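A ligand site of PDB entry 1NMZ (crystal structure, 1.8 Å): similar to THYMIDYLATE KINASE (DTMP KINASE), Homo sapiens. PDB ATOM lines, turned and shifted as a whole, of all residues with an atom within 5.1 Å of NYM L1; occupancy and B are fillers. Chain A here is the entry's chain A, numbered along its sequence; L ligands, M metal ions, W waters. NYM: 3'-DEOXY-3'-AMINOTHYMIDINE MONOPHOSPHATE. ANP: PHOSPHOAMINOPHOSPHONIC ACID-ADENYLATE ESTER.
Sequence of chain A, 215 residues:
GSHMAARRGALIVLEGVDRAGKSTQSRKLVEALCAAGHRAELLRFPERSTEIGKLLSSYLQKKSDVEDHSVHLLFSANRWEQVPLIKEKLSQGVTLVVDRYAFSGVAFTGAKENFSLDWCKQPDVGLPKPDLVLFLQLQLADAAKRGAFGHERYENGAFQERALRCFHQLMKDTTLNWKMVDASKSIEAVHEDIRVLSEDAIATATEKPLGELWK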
ATOM      1  N   ASP A  18      30.622   2.249  32.766  1.00  0.00           N
ATOM      2  CA  ASP A  18      29.355   2.946  32.464  1.00  0.00           C
ATOM      3  C   ASP A  18      29.593   4.436  32.243  1.00  0.00           C
ATOM      4  O   ASP A  18      30.361   5.188  32.833  1.00  0.00           O
ATOM      5  CB  ASP A  18      28.339   2.684  33.590  1.00  0.00           C
ATOM      6  CG  ASP A  18      28.065   1.201  33.755  1.00  0.00           C
ATOM      7  OD1 ASP A  18      28.203   0.411  32.802  1.00  0.00           O
ATOM      8  OD2 ASP A  18      27.683   0.716  34.836  1.00  0.00           O
ATOM      9  N   LYS A  22      30.228   4.572  25.129  1.00  0.00           N
ATOM     10  CA  LYS A  22      30.212   3.419  24.233  1.00  0.00           C
ATOM     11  C   LYS A  22      29.089   3.401  23.204  1.00  0.00           C
ATOM     12  O   LYS A  22      29.276   3.101  22.017  1.00  0.00           O
ATOM     13  CB  LYS A  22      30.175   2.114  25.057  1.00  0.00           C
ATOM     14  CG  LYS A  22      31.410   2.074  26.006  1.00  0.00           C
ATOM     15  CD  LYS A  22      31.306   0.780  26.864  1.00  0.00           C
ATOM     16  CE  LYS A  22      30.018   0.705  27.677  1.00  0.00           C
ATOM     17  NZ  LYS A  22      29.947   1.773  28.729  1.00  0.00           N
ATOM     18  N   PHE A  45      25.757  -5.877  23.574  1.00  0.00           N
ATOM     19  CA  PHE A  45      25.532  -6.880  24.603  1.00  0.00           C
ATOM     20  C   PHE A  45      25.345  -6.137  25.912  1.00  0.00           C
ATOM     21  O   PHE A  45      26.061  -5.165  26.236  1.00  0.00           O
ATOM     22  CB  PHE A  45      26.705  -7.887  24.665  1.00  0.00           C
ATOM     23  CG  PHE A  45      26.691  -8.748  23.425  1.00  0.00           C
ATOM     24  CD1 PHE A  45      27.624  -8.533  22.420  1.00  0.00           C
ATOM     25  CD2 PHE A  45      25.715  -9.732  23.242  1.00  0.00           C
ATOM     26  CE1 PHE A  45      27.595  -9.290  21.262  1.00  0.00           C
ATOM     27  CE2 PHE A  45      25.671 -10.494  22.078  1.00  0.00           C
ATOM     28  CZ  PHE A  45      26.628 -10.264  21.081  1.00  0.00           C
ATOM     29  N   PRO A  46      24.393  -6.560  26.729  1.00  0.00           N
ATOM     30  CA  PRO A  46      23.464  -7.627  26.409  1.00  0.00           C
ATOM     31  C   PRO A  46      22.534  -7.267  25.274  1.00  0.00           C
ATOM     32  O   PRO A  46      22.173  -6.084  25.090  1.00  0.00           O
ATOM     33  CB  PRO A  46      22.626  -7.804  27.690  1.00  0.00           C
ATOM     34  CG  PRO A  46      22.701  -6.464  28.309  1.00  0.00           C
ATOM     35  CD  PRO A  46      24.063  -5.906  28.019  1.00  0.00           C
ATOM     36  N   ARG A  48      19.030  -7.537  24.489  1.00  0.00           N
ATOM     37  CA  ARG A  48      17.819  -7.834  25.270  1.00  0.00           C
ATOM     38  C   ARG A  48      16.630  -8.382  24.549  1.00  0.00           C
ATOM     39  O   ARG A  48      15.635  -8.700  25.242  1.00  0.00           O
ATOM     40  CB  ARG A  48      17.446  -6.556  26.052  1.00  0.00           C
ATOM     41  CG  ARG A  48      18.618  -6.038  26.871  1.00  0.00           C
ATOM     42  CD  ARG A  48      18.267  -4.756  27.591  1.00  0.00           C
ATOM     43  NE  ARG A  48      19.429  -4.077  28.167  1.00  0.00           N
ATOM     44  CZ  ARG A  48      19.319  -3.523  29.378  1.00  0.00           C
ATOM     45  NH1 ARG A  48      18.172  -3.630  30.033  1.00  0.00           N
ATOM     46  NH2 ARG A  48      20.354  -2.899  29.936  1.00  0.00           N
ATOM     47  N   LEU A  60      18.952  -6.488  35.448  1.00  0.00           N
ATOM     48  CA  LEU A  60      19.633  -5.202  35.492  1.00  0.00           C
ATOM     49  C   LEU A  60      18.738  -4.111  36.057  1.00  0.00           C
ATOM     50  O   LEU A  60      19.257  -3.203  36.721  1.00  0.00           O
ATOM     51  CB  LEU A  60      20.167  -4.852  34.082  1.00  0.00           C
ATOM     52  CG  LEU A  60      21.383  -5.723  33.697  1.00  0.00           C
ATOM     53  CD1 LEU A  60      21.702  -5.592  32.206  1.00  0.00           C
ATOM     54  CD2 LEU A  60      22.592  -5.347  34.552  1.00  0.00           C
ATOM     55  N   PHE A  75      24.743 -14.007  30.785  1.00  0.00           N
ATOM     56  CA  PHE A  75      25.380 -12.972  29.920  1.00  0.00           C
ATOM     57  C   PHE A  75      26.207 -13.575  28.785  1.00  0.00           C
ATOM     58  O   PHE A  75      26.296 -13.078  27.678  1.00  0.00           O
ATOM     59  CB  PHE A  75      26.261 -12.023  30.749  1.00  0.00           C
ATOM     60  CG  PHE A  75      25.516 -10.841  31.344  1.00  0.00           C
ATOM     61  CD1 PHE A  75      25.310 -10.750  32.726  1.00  0.00           C
ATOM     62  CD2 PHE A  75      25.047  -9.810  30.508  1.00  0.00           C
ATOM     63  CE1 PHE A  75      24.632  -9.654  33.254  1.00  0.00           C
ATOM     64  CE2 PHE A  75      24.374  -8.719  31.043  1.00  0.00           C
ATOM     65  CZ  PHE A  75      24.159  -8.640  32.424  1.00  0.00           C
ATOM     66  N   ARG A  79      25.798 -13.990  24.380  1.00  0.00           N
ATOM     67  CA  ARG A  79      26.766 -13.755  23.302  1.00  0.00           C
ATOM     68  C   ARG A  79      26.811 -14.972  22.379  1.00  0.00           C
ATOM     69  O   ARG A  79      26.750 -14.771  21.166  1.00  0.00           O
ATOM     70  CB  ARG A  79      28.187 -13.465  23.833  1.00  0.00           C
ATOM     71  CG  ARG A  79      28.293 -12.032  24.366  1.00  0.00           C
ATOM     72  CD  ARG A  79      29.692 -11.900  24.968  1.00  0.00           C
ATOM     73  NE  ARG A  79      29.893 -12.421  26.309  1.00  0.00           N
ATOM     74  CZ  ARG A  79      29.464 -11.887  27.458  1.00  0.00           C
ATOM     75  NH1 ARG A  79      28.667 -10.790  27.487  1.00  0.00           N
ATOM     76  NH2 ARG A  79      29.821 -12.406  28.641  1.00  0.00           N
ATOM     77  N   ASP A  99      28.846  -2.965  20.864  1.00  0.00           N
ATOM     78  CA  ASP A  99      28.792  -2.155  22.086  1.00  0.00           C
ATOM     79  C   ASP A  99      28.762  -3.072  23.320  1.00  0.00           C
ATOM     80  O   ASP A  99      27.674  -3.604  23.620  1.00  0.00           O
ATOM     81  CB  ASP A  99      27.534  -1.305  21.950  1.00  0.00           C
ATOM     82  CG  ASP A  99      27.240  -0.345  23.080  1.00  0.00           C
ATOM     83  OD1 ASP A  99      27.973  -0.196  24.077  1.00  0.00           O
ATOM     84  OD2 ASP A  99      26.091   0.200  22.987  1.00  0.00           O
ATOM     85  N   ARG A 100      29.919  -3.292  23.876  1.00  0.00           N
ATOM     86  CA  ARG A 100      30.229  -4.194  24.965  1.00  0.00           C
ATOM     87  C   ARG A 100      30.344  -5.640  24.456  1.00  0.00           C
ATOM     88  O   ARG A 100      29.616  -6.028  23.518  1.00  0.00           O
ATOM     89  CB  ARG A 100      29.279  -4.216  26.190  1.00  0.00           C
ATOM     90  CG  ARG A 100      29.233  -2.819  26.894  1.00  0.00           C
ATOM     91  CD  ARG A 100      28.462  -3.128  28.226  1.00  0.00           C
ATOM     92  NE  ARG A 100      28.159  -1.995  29.060  1.00  0.00           N
ATOM     93  CZ  ARG A 100      28.970  -1.550  30.022  1.00  0.00           C
ATOM     94  NH1 ARG A 100      30.166  -2.080  30.260  1.00  0.00           N
ATOM     95  NH2 ARG A 100      28.529  -0.490  30.710  1.00  0.00           N
ATOM     96  N   TYR A 101      31.207  -6.412  25.089  1.00  0.00           N
ATOM     97  CA  TYR A 101      31.361  -7.825  24.699  1.00  0.00           C
ATOM     98  C   TYR A 101      31.792  -8.645  25.908  1.00  0.00           C
ATOM     99  O   TYR A 101      31.443  -8.339  27.049  1.00  0.00           O
ATOM    100  CB  TYR A 101      32.335  -7.947  23.550  1.00  0.00           C
ATOM    101  CG  TYR A 101      32.409  -9.195  22.700  1.00  0.00           C
ATOM    102  CD1 TYR A 101      31.300  -9.736  22.057  1.00  0.00           C
ATOM    103  CD2 TYR A 101      33.642  -9.814  22.479  1.00  0.00           C
ATOM    104  CE1 TYR A 101      31.399 -10.835  21.218  1.00  0.00           C
ATOM    105  CE2 TYR A 101      33.728 -10.919  21.616  1.00  0.00           C
ATOM    106  CZ  TYR A 101      32.633 -11.437  21.026  1.00  0.00           C
ATOM    107  OH  TYR A 101      32.717 -12.521  20.150  1.00  0.00           O
ATOM    108  N   SER A 104      33.347  -6.851  29.238  1.00  0.00           N
ATOM    109  CA  SER A 104      32.373  -6.302  30.202  1.00  0.00           C
ATOM    110  C   SER A 104      31.859  -7.470  31.072  1.00  0.00           C
ATOM    111  O   SER A 104      31.647  -7.332  32.283  1.00  0.00           O
ATOM    112  CB  SER A 104      31.160  -5.693  29.491  1.00  0.00           C
ATOM    113  OG  SER A 104      31.446  -4.310  29.219  1.00  0.00           O
ATOM    114  N   GLY A 105      31.660  -8.606  30.417  1.00  0.00           N
ATOM    115  CA  GLY A 105      31.139  -9.759  31.181  1.00  0.00           C
ATOM    116  C   GLY A 105      32.117 -10.097  32.326  1.00  0.00           C
ATOM    117  O   GLY A 105      31.673 -10.459  33.421  1.00  0.00           O
ATOM    118  N   PHE A 108      32.533  -7.069  35.093  1.00  0.00           N
ATOM    119  CA  PHE A 108      31.418  -6.828  35.980  1.00  0.00           C
ATOM    120  C   PHE A 108      31.292  -7.949  37.000  1.00  0.00           C
ATOM    121  O   PHE A 108      31.114  -7.639  38.187  1.00  0.00           O
ATOM    122  CB  PHE A 108      30.149  -6.470  35.199  1.00  0.00           C
ATOM    123  CG  PHE A 108      30.224  -4.993  34.839  1.00  0.00           C
ATOM    124  CD1 PHE A 108      30.985  -4.576  33.759  1.00  0.00           C
ATOM    125  CD2 PHE A 108      29.554  -4.044  35.593  1.00  0.00           C
ATOM    126  CE1 PHE A 108      31.064  -3.222  33.449  1.00  0.00           C
ATOM    127  CE2 PHE A 108      29.637  -2.703  35.283  1.00  0.00           C
ATOM    128  CZ  PHE A 108      30.407  -2.276  34.204  1.00  0.00           C
ATOM    129  N   GLU A 152      20.001   1.544  37.476  1.00  0.00           N
ATOM    130  CA  GLU A 152      20.240   0.133  37.171  1.00  0.00           C
ATOM    131  C   GLU A 152      21.307  -0.480  38.076  1.00  0.00           C
ATOM    132  O   GLU A 152      22.134   0.187  38.686  1.00  0.00           O
ATOM    133  CB  GLU A 152      20.560  -0.142  35.695  1.00  0.00           C
ATOM    134  CG  GLU A 152      19.407  -0.049  34.707  1.00  0.00           C
ATOM    135  CD  GLU A 152      19.560  -0.910  33.467  1.00  0.00           C
ATOM    136  OE1 GLU A 152      20.695  -1.273  33.078  1.00  0.00           O
ATOM    137  OE2 GLU A 152      18.536  -1.269  32.828  1.00  0.00           O
ATOM    138  N   ARG A 153      21.299  -1.805  38.137  1.00  0.00           N
ATOM    139  CA  ARG A 153      22.267  -2.534  38.966  1.00  0.00           C
ATOM    140  C   ARG A 153      23.689  -2.116  38.634  1.00  0.00           C
ATOM    141  O   ARG A 153      23.966  -1.816  37.471  1.00  0.00           O
ATOM    142  CB  ARG A 153      22.077  -4.036  38.722  1.00  0.00           C
ATOM    143  CG  ARG A 153      22.039  -4.826  40.021  1.00  0.00           C
ATOM    144  CD  ARG A 153      21.877  -6.305  39.774  1.00  0.00           C
ATOM    145  NE  ARG A 153      20.513  -6.803  39.684  1.00  0.00           N
ATOM    146  CZ  ARG A 153      19.734  -7.057  40.729  1.00  0.00           C
ATOM    147  NH1 ARG A 153      20.225  -6.836  41.954  1.00  0.00           N
ATOM    148  NH2 ARG A 153      18.518  -7.534  40.596  1.00  0.00           N
ATOM    149  N   TYR A 154      24.586  -2.088  39.610  1.00  0.00           N
ATOM    150  CA  TYR A 154      25.985  -1.761  39.377  1.00  0.00           C
ATOM    151  C   TYR A 154      26.277  -0.274  39.185  1.00  0.00           C
ATOM    152  O   TYR A 154      27.459   0.064  39.016  1.00  0.00           O
ATOM    153  CB  TYR A 154      26.524  -2.496  38.140  1.00  0.00           C
ATOM    154  CG  TYR A 154      26.382  -3.988  38.081  1.00  0.00           C
ATOM    155  CD1 TYR A 154      26.358  -4.658  36.852  1.00  0.00           C
ATOM    156  CD2 TYR A 154      26.247  -4.764  39.224  1.00  0.00           C
ATOM    157  CE1 TYR A 154      26.236  -6.041  36.776  1.00  0.00           C
ATOM    158  CE2 TYR A 154      26.119  -6.133  39.164  1.00  0.00           C
ATOM    159  CZ  TYR A 154      26.113  -6.782  37.954  1.00  0.00           C
ATOM    160  OH  TYR A 154      25.991  -8.157  37.883  1.00  0.00           O
HETATM  161  N1  NYM L   1      27.108  -6.249  31.826  1.00  0.00           N
HETATM  162  C6  NYM L   1      27.141  -6.220  30.470  1.00  0.00           C
HETATM  163  C2  NYM L   1      27.411  -7.392  32.612  1.00  0.00           C
HETATM  164  O2  NYM L   1      27.330  -7.339  33.845  1.00  0.00           O
HETATM  165  N3  NYM L   1      27.862  -8.471  31.932  1.00  0.00           N
HETATM  166  C4  NYM L   1      27.948  -8.517  30.531  1.00  0.00           C
HETATM  167  O4  NYM L   1      28.356  -9.674  30.004  1.00  0.00           O
HETATM  168  C5  NYM L   1      27.567  -7.285  29.775  1.00  0.00           C
HETATM  169  C7  NYM L   1      27.702  -7.435  28.248  1.00  0.00           C
HETATM  170  O4' NYM L   1      25.320  -4.851  31.934  1.00  0.00           O
HETATM  171  N3' NYM L   1      26.101  -2.104  33.661  1.00  0.00           N
HETATM  172  C1' NYM L   1      26.523  -5.048  32.518  1.00  0.00           C
HETATM  173  C2' NYM L   1      27.255  -3.720  32.248  1.00  0.00           C
HETATM  174  C3' NYM L   1      26.161  -2.664  32.241  1.00  0.00           C
HETATM  175  C4' NYM L   1      24.893  -3.519  32.129  1.00  0.00           C
HETATM  176  O5' NYM L   1      24.866  -2.427  29.997  1.00  0.00           O
HETATM  177  C5' NYM L   1      23.950  -2.909  31.028  1.00  0.00           C
HETATM  178  P1  NYM L   1      24.485  -1.287  28.918  1.00  0.00           P
HETATM  179  OP2 NYM L   1      23.746  -0.106  29.444  1.00  0.00           O
HETATM  180  OP1 NYM L   1      25.682  -1.242  28.078  1.00  0.00           O
HETATM  181  OP3 NYM L   1      23.144  -2.072  28.355  1.00  0.00           O
HETATM  182  PG  ANP L   2      26.337   2.747  29.540  1.00  0.00           P
HETATM  183  O1G ANP L   2      25.539   3.114  30.777  1.00  0.00           O
HETATM  184  O2G ANP L   2      25.451   2.060  28.622  1.00  0.00           O
HETATM  185  O3G ANP L   2      27.591   2.011  29.881  1.00  0.00           O
HETATM  186  PB  ANP L   2      27.593   4.516  27.542  1.00  0.00           P
HETATM  187  O1B ANP L   2      29.003   4.389  27.723  1.00  0.00           O
HETATM  188  O2B ANP L   2      26.953   3.655  26.556  1.00  0.00           O
HETATM  189  N3B ANP L   2      26.775   4.268  29.025  1.00  0.00           N
HETATM  190  PA  ANP L   2      26.451   6.858  26.319  1.00  0.00           P
HETATM  191  O1A ANP L   2      27.044   6.843  24.941  1.00  0.00           O
HETATM  192  O2A ANP L   2      25.075   6.354  26.448  1.00  0.00           O
HETATM  193  O3A ANP L   2      27.459   6.090  27.297  1.00  0.00           O
HETATM  194  O5' ANP L   2      26.584   8.331  26.876  1.00  0.00           O
HETATM  195  C5' ANP L   2      26.196   8.626  28.286  1.00  0.00           C
HETATM  196  C4' ANP L   2      25.741  10.081  28.329  1.00  0.00           C
HETATM  197  O4' ANP L   2      26.879  10.920  28.196  1.00  0.00           O
HETATM  198  C3' ANP L   2      24.799  10.490  27.198  1.00  0.00           C
HETATM  199  O3' ANP L   2      23.912  11.584  27.635  1.00  0.00           O
HETATM  200  C2' ANP L   2      25.703  11.033  26.136  1.00  0.00           C
HETATM  201  O2' ANP L   2      25.079  12.053  25.296  1.00  0.00           O
HETATM  202  C1' ANP L   2      26.783  11.710  26.993  1.00  0.00           C
HETATM  203  N9  ANP L   2      28.100  11.683  26.301  1.00  0.00           N
HETATM  204  C8  ANP L   2      28.590  10.746  25.429  1.00  0.00           C
HETATM  205  N7  ANP L   2      29.800  11.019  24.998  1.00  0.00           N
HETATM  206  C5  ANP L   2      30.102  12.220  25.592  1.00  0.00           C
HETATM  207  C6  ANP L   2      31.252  13.043  25.512  1.00  0.00           C
HETATM  208  N6  ANP L   2      32.324  12.728  24.738  1.00  0.00           N
HETATM  209  N1  ANP L   2      31.228  14.159  26.242  1.00  0.00           N
HETATM  210  C2  ANP L   2      30.155  14.458  26.987  1.00  0.00           C
HETATM  211  N3  ANP L   2      29.035  13.774  27.143  1.00  0.00           N
HETATM  212  C4  ANP L   2      29.085  12.636  26.404  1.00  0.00           C
HETATM  213 MG    MG M   1      25.506   2.292  26.555  1.00  0.00          MG
HETATM  214  O   HOH W   1      22.730  -3.589  25.824  1.00  0.00           O
HETATM  215  O   HOH W   2      23.779   0.979  26.365  1.00  0.00           O
HETATM  216  O   HOH W   3      27.635  -9.260  35.923  1.00  0.00           O
HETATM  217  O   HOH W   4      24.019  -1.618  34.824  1.00  0.00           O
HETATM  218  O   HOH W   5      25.415  -2.557  25.685  1.00  0.00           O
HETATM  219  O   HOH W   6      26.855   0.654  26.302  1.00  0.00           O
HETATM  220  O   HOH W   7      28.693 -10.797  33.302  1.00  0.00           O
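The guanidinium group (NE) of Arg 100 is in salt-bridge range of an oxygen (OP1) of NYM L1, 2.8 Å away. NH1 of Arg 79 lies within hydrogen-bond range of O4 of NYM L1 (2.8 Å). N of Gly 105 sits close to O4 of NYM L1. An oxygen (OP3) of NYM L1 lies within salt-bridge range of the guanidinium group of Arg 48 (3.3 Å). The side-chain carboxylate (OD1) of Asp 18 is in salt-bridge range of a nitrogen (N3') of NYM L1. An oxygen (O3G) of ANP L2 lies within salt-bridge range of the guanidinium group (NH2) of Arg 100, at 2.8 Å. N of Lys 22 lies within hydrogen-bond range of O1B of ANP L2. NZ of Lys 22 lies within salt-bridge range of O3G of ANP L2, at 2.6 Å.
An oxygen (O2G) of ANP L2 lies close to an oxygen (OP2) of NYM L1, at 2.9 Å.
NH1 of Arg 100 lies within hydrogen-bond range of OG of Ser 104 (2.8 Å). The backbone carbonyl oxygen of Phe 75 is in hydrogen-bond range of the guanidinium group of Arg 79 (3.3 Å). The side-chain carboxylate (OE1) of Glu 152 is in salt-bridge range of the guanidinium group (NH2) of Arg 48 (3.6 Å). The backbone NH (N) of Phe 45 sits at hydrogen-bond distance from the backbone carbonyl oxygen (O) of Asp 99 (3.0 Å). N of Arg 153 sits at hydrogen-bond distance from O of Leu 60, 2.9 Å away.
Phe 45 touches NYM L1 (O to C7, 3.4 Å). Pro 46 touches NYM L1. CD1 of Leu 60 touches C5' of NYM L1, 3.7 Å away. CD2 of Phe 75 touches C4 of NYM L1, at 3.2 Å. Ser 104 touches NYM L1 (CB to C5, 3.9 Å). CB of Phe 108 touches O2 of NYM L1, 3.2 Å away. CE1 of Tyr 154 touches O2 of NYM L1 (3.4 Å). Hydrophobic or aromatic side chains that line NYM L1: Phe 45, Pro 46, Leu 60, Phe 75, Phe 108 and Tyr 154. 12 residues have an atom within 4 Å of NYM L1: Asp 18, Phe 45, Pro 46, Arg 48, Leu 60, Phe 75, Arg 79, Arg 100, Ser 104, Gly 105, Phe 108 and Tyr 154. The nearest printed residue that does not touch NYM L1 is Tyr 101 (4.03 Å).
Water W4 bridges N3' of NYM L1 and O of Arg 153. Water W5 lies within hydrogen-bond range of O of Phe 45 (2.7 Å), OP1 of NYM L1 (2.7 Å) and O of Asp 99 (3.2 Å). Water W7 lies within hydrogen-bond range of N3 of NYM L1 and O of Gly 105. Water W3 lies within hydrogen-bond range of the side-chain hydroxyl (OH) of Tyr 154 and an oxygen (O2) of NYM L1. Water W6 lies within hydrogen-bond range of the side-chain carboxylate (OD1) of Asp 99 (2.6 Å) and an oxygen (OP1) of NYM L1 (2.9 Å). Water W1 bridges O of Pro 46 (2.7 Å) and OP3 of NYM L1 (3.0 Å).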
